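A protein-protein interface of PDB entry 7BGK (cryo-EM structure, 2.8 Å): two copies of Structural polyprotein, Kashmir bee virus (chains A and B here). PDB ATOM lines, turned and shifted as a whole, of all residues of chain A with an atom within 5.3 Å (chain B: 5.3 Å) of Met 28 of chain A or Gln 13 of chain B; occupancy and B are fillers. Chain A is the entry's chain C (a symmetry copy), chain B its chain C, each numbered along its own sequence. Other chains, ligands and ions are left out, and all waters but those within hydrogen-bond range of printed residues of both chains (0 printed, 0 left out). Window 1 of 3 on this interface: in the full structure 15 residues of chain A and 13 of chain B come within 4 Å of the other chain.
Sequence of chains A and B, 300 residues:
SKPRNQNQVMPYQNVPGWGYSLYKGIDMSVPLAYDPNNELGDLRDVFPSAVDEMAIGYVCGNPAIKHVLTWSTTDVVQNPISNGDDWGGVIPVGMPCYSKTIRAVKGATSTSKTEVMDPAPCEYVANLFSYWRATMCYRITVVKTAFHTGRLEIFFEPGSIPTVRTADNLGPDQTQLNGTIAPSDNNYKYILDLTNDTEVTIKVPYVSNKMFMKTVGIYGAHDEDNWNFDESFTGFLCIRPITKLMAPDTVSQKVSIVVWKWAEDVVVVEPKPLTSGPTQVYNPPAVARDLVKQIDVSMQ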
ATOM      1  N   ASN A  14      27.498 -14.170  31.768  1.00  0.00           N
ATOM      2  CA  ASN A  14      26.465 -14.765  30.918  1.00  0.00           C
ATOM      3  C   ASN A  14      25.104 -14.276  31.395  1.00  0.00           C
ATOM      4  O   ASN A  14      24.384 -14.942  32.138  1.00  0.00           O
ATOM      5  CB  ASN A  14      26.549 -16.282  30.945  1.00  0.00           C
ATOM      6  CG  ASN A  14      25.802 -16.923  29.807  1.00  0.00           C
ATOM      7  OD1 ASN A  14      25.040 -16.275  29.098  1.00  0.00           O
ATOM      8  ND2 ASN A  14      26.013 -18.213  29.630  1.00  0.00           N
ATOM      9  N   VAL A  15      24.732 -13.098  30.912  1.00  0.00           N
ATOM     10  CA  VAL A  15      23.536 -12.418  31.390  1.00  0.00           C
ATOM     11  C   VAL A  15      22.630 -12.049  30.219  1.00  0.00           C
ATOM     12  O   VAL A  15      22.693 -10.927  29.701  1.00  0.00           O
ATOM     13  CB  VAL A  15      23.924 -11.203  32.251  1.00  0.00           C
ATOM     14  CG1 VAL A  15      24.772 -10.217  31.475  1.00  0.00           C
ATOM     15  CG2 VAL A  15      22.695 -10.532  32.806  1.00  0.00           C
ATOM     16  N   PRO A  16      21.776 -12.964  29.773  1.00  0.00           N
ATOM     17  CA  PRO A  16      20.789 -12.609  28.755  1.00  0.00           C
ATOM     18  C   PRO A  16      19.717 -11.697  29.323  1.00  0.00           C
ATOM     19  O   PRO A  16      19.325 -11.806  30.487  1.00  0.00           O
ATOM     20  CB  PRO A  16      20.205 -13.963  28.336  1.00  0.00           C
ATOM     21  CG  PRO A  16      21.066 -14.992  28.944  1.00  0.00           C
ATOM     22  CD  PRO A  16      21.709 -14.386  30.124  1.00  0.00           C
ATOM     23  N   GLY A  17      19.238 -10.791  28.480  1.00  0.00           N
ATOM     24  CA  GLY A  17      18.258  -9.821  28.915  1.00  0.00           C
ATOM     25  C   GLY A  17      18.817  -8.801  29.880  1.00  0.00           C
ATOM     26  O   GLY A  17      18.262  -8.591  30.962  1.00  0.00           O
ATOM     27  N   ILE A  26      20.300  -1.320  22.750  1.00  0.00           N
ATOM     28  CA  ILE A  26      20.282  -2.177  21.576  1.00  0.00           C
ATOM     29  C   ILE A  26      19.650  -3.506  21.963  1.00  0.00           C
ATOM     30  O   ILE A  26      20.195  -4.250  22.785  1.00  0.00           O
ATOM     31  CB  ILE A  26      21.697  -2.367  21.012  1.00  0.00           C
ATOM     32  CG1 ILE A  26      22.239  -1.025  20.517  1.00  0.00           C
ATOM     33  CG2 ILE A  26      21.688  -3.366  19.898  1.00  0.00           C
ATOM     34  CD1 ILE A  26      23.699  -1.007  20.248  1.00  0.00           C
ATOM     35  N   ASP A  27      18.493  -3.799  21.378  1.00  0.00           N
ATOM     36  CA  ASP A  27      17.733  -4.991  21.708  1.00  0.00           C
ATOM     37  C   ASP A  27      18.213  -6.186  20.902  1.00  0.00           C
ATOM     38  O   ASP A  27      18.484  -6.080  19.704  1.00  0.00           O
ATOM     39  CB  ASP A  27      16.247  -4.773  21.446  1.00  0.00           C
ATOM     40  CG  ASP A  27      15.368  -5.580  22.374  1.00  0.00           C
ATOM     41  OD1 ASP A  27      15.804  -6.658  22.826  1.00  0.00           O
ATOM     42  OD2 ASP A  27      14.237  -5.136  22.650  1.00  0.00           O
ATOM     43  N   MET A  28      18.296  -7.332  21.572  1.00  0.00           N
ATOM     44  CA  MET A  28      18.705  -8.577  20.953  1.00  0.00           C
ATOM     45  C   MET A  28      17.521  -9.397  20.477  1.00  0.00           C
ATOM     46  O   MET A  28      17.624 -10.623  20.368  1.00  0.00           O
ATOM     47  CB  MET A  28      19.557  -9.381  21.926  1.00  0.00           C
ATOM     48  CG  MET A  28      20.899  -8.750  22.196  1.00  0.00           C
ATOM     49  SD  MET A  28      21.938  -8.647  20.740  1.00  0.00           S
ATOM     50  CE  MET A  28      22.135 -10.377  20.376  1.00  0.00           C
ATOM     51  N   SER A  29      16.401  -8.746  20.196  1.00  0.00           N
ATOM     52  CA  SER A  29      15.206  -9.425  19.729  1.00  0.00           C
ATOM     53  C   SER A  29      15.334  -9.749  18.249  1.00  0.00           C
ATOM     54  O   SER A  29      15.463  -8.844  17.418  1.00  0.00           O
ATOM     55  CB  SER A  29      13.980  -8.562  19.995  1.00  0.00           C
ATOM     56  OG  SER A  29      13.760  -8.413  21.383  1.00  0.00           O
ATOM     57  N   VAL A  30      15.294 -11.032  17.922  1.00  0.00           N
ATOM     58  CA  VAL A  30      15.459 -11.460  16.531  1.00  0.00           C
ATOM     59  C   VAL A  30      14.205 -11.105  15.744  1.00  0.00           C
ATOM     60  O   VAL A  30      13.088 -11.412  16.192  1.00  0.00           O
ATOM     61  CB  VAL A  30      15.729 -12.960  16.472  1.00  0.00           C
ATOM     62  CG1 VAL A  30      15.911 -13.411  15.059  1.00  0.00           C
ATOM     63  CG2 VAL A  30      16.931 -13.308  17.275  1.00  0.00           C
ATOM     64  N   PRO B  11      28.608  -8.148  28.602  1.00  0.00           N
ATOM     65  CA  PRO B  11      27.343  -8.882  28.654  1.00  0.00           C
ATOM     66  C   PRO B  11      27.139  -9.676  27.372  1.00  0.00           C
ATOM     67  O   PRO B  11      27.899  -9.562  26.412  1.00  0.00           O
ATOM     68  CB  PRO B  11      26.305  -7.776  28.800  1.00  0.00           C
ATOM     69  CG  PRO B  11      26.896  -6.647  28.100  1.00  0.00           C
ATOM     70  CD  PRO B  11      28.382  -6.733  28.269  1.00  0.00           C
ATOM     71  N   TYR B  12      26.091 -10.492  27.365  1.00  0.00           N
ATOM     72  CA  TYR B  12      26.102 -11.600  26.424  1.00  0.00           C
ATOM     73  C   TYR B  12      24.831 -12.441  26.454  1.00  0.00           C
ATOM     74  O   TYR B  12      24.037 -12.398  27.396  1.00  0.00           O
ATOM     75  CB  TYR B  12      27.313 -12.420  26.769  1.00  0.00           C
ATOM     76  CG  TYR B  12      27.392 -13.763  26.171  1.00  0.00           C
ATOM     77  CD1 TYR B  12      28.214 -14.020  25.108  1.00  0.00           C
ATOM     78  CD2 TYR B  12      26.670 -14.801  26.715  1.00  0.00           C
ATOM     79  CE1 TYR B  12      28.304 -15.269  24.606  1.00  0.00           C
ATOM     80  CE2 TYR B  12      26.752 -16.051  26.218  1.00  0.00           C
ATOM     81  CZ  TYR B  12      27.572 -16.288  25.175  1.00  0.00           C
ATOM     82  OH  TYR B  12      27.608 -17.566  24.721  1.00  0.00           O
ATOM     83  N   GLN B  13      24.688 -13.242  25.398  1.00  0.00           N
ATOM     84  CA  GLN B  13      23.612 -14.197  25.194  1.00  0.00           C
ATOM     85  C   GLN B  13      24.178 -15.319  24.338  1.00  0.00           C
ATOM     86  O   GLN B  13      24.801 -15.048  23.309  1.00  0.00           O
ATOM     87  CB  GLN B  13      22.418 -13.536  24.505  1.00  0.00           C
ATOM     88  CG  GLN B  13      21.176 -14.362  24.442  1.00  0.00           C
ATOM     89  CD  GLN B  13      20.040 -13.634  23.775  1.00  0.00           C
ATOM     90  OE1 GLN B  13      20.165 -13.168  22.645  1.00  0.00           O
ATOM     91  NE2 GLN B  13      18.920 -13.533  24.466  1.00  0.00           N
ATOM     92  N   ASN B  14      23.985 -16.569  24.763  1.00  0.00           N
ATOM     93  CA  ASN B  14      24.491 -17.718  24.008  1.00  0.00           C
ATOM     94  C   ASN B  14      23.427 -18.143  23.004  1.00  0.00           C
ATOM     95  O   ASN B  14      22.648 -19.070  23.220  1.00  0.00           O
ATOM     96  CB  ASN B  14      24.861 -18.858  24.940  1.00  0.00           C
ATOM     97  CG  ASN B  14      25.744 -19.882  24.280  1.00  0.00           C
ATOM     98  OD1 ASN B  14      25.929 -19.877  23.067  1.00  0.00           O
ATOM     99  ND2 ASN B  14      26.290 -20.776  25.080  1.00  0.00           N
ATOM    100  N   VAL B  15      23.434 -17.471  21.861  1.00  0.00           N
ATOM    101  CA  VAL B  15      22.387 -17.645  20.865  1.00  0.00           C
ATOM    102  C   VAL B  15      22.997 -17.973  19.505  1.00  0.00           C
ATOM    103  O   VAL B  15      23.215 -17.079  18.678  1.00  0.00           O
ATOM    104  CB  VAL B  15      21.476 -16.405  20.827  1.00  0.00           C
ATOM    105  CG1 VAL B  15      22.258 -15.148  20.503  1.00  0.00           C
ATOM    106  CG2 VAL B  15      20.351 -16.603  19.846  1.00  0.00           C
ATOM    107  N   TRP B  18      21.665 -16.617  15.111  1.00  0.00           N
ATOM    108  CA  TRP B  18      20.926 -15.377  15.304  1.00  0.00           C
ATOM    109  C   TRP B  18      20.665 -14.749  13.942  1.00  0.00           C
ATOM    110  O   TRP B  18      21.592 -14.269  13.283  1.00  0.00           O
ATOM    111  CB  TRP B  18      21.706 -14.423  16.199  1.00  0.00           C
ATOM    112  CG  TRP B  18      20.905 -13.286  16.744  1.00  0.00           C
ATOM    113  CD1 TRP B  18      20.420 -13.167  18.003  1.00  0.00           C
ATOM    114  CD2 TRP B  18      20.503 -12.102  16.048  1.00  0.00           C
ATOM    115  NE1 TRP B  18      19.740 -11.990  18.143  1.00  0.00           N
ATOM    116  CE2 TRP B  18      19.777 -11.313  16.954  1.00  0.00           C
ATOM    117  CE3 TRP B  18      20.684 -11.632  14.747  1.00  0.00           C
ATOM    118  CZ2 TRP B  18      19.229 -10.091  16.601  1.00  0.00           C
ATOM    119  CZ3 TRP B  18      20.144 -10.422  14.405  1.00  0.00           C
ATOM    120  CH2 TRP B  18      19.425  -9.663  15.324  1.00  0.00           C
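O of Met 28 of chain A lies within hydrogen-bond range of NE1 of Trp 18 of chain B (3.4 Å). O of Tyr 12 of chain B lies close to O of Val 15 of chain A (3.0 Å). The backbone nitrogen (N) of Pro 16 of chain A lies close to the backbone carbonyl oxygen (O) of Tyr 12 of chain B, at 3.3 Å.
The side-chain hydroxyl of Tyr 12 of chain B sits close to the side-chain amide oxygen of Asn 14 of chain B, 3.3 Å away.
OD1 of Asn 14 of chain A touches CD2 of Tyr 12 of chain B, 3.2 Å away. CG1 of Val 15 of chain A touches CB of Pro 11 of chain B, 3.9 Å away. OE1 of Gln 13 of chain B touches CB of Met 28 of chain A, 3.9 Å away. CG2 of Val 30 of chain A touches NE1 of Trp 18 of chain B, at 3.2 Å.
Printed residues of chain B within 4 Å of Met 28 of chain A: Gln 13 and Trp 18. Gln 13 of chain B touches one residue of chain A. Of the printed residues of chain A, Trp 18 of chain B touches Met 28 (3.4 Å) and Val 30 (3.2 Å). Of the printed residues of chain B, Val 30 of chain A touches Trp 18. Printed residues of chain B within 4 Å of Val 15 of chain A: Pro 11 and Tyr 12. Gly 17 of chain A touches none of the printed residues of chain B. The nearest printed residue of chain A that does not touch Pro 11 of chain B is Asn 14 of chain A (6.1 Å).
Of the 9 printed residues of chain A, 5 touch a printed residue of chain B. Hydrophobic or aromatic side chains of chain A within 4 Å of the printed part of chain B: Val 15, Met 28 and Val 30. Printed residues of chain B that touch a printed residue of chain A: Pro 11, Tyr 12, Gln 13 and Trp 18. Hydrophobic or aromatic side chains of chain B within 4 Å of the printed part of chain A: Pro 11, Tyr 12 and Trp 18. Among the printed residues, 7 pairs touch across the chains.
Positions printed for both chains: 14 and 15. Of the 7 pairs that touch across the chains among the printed residues, none has its exchanged pair printed and touching as well.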
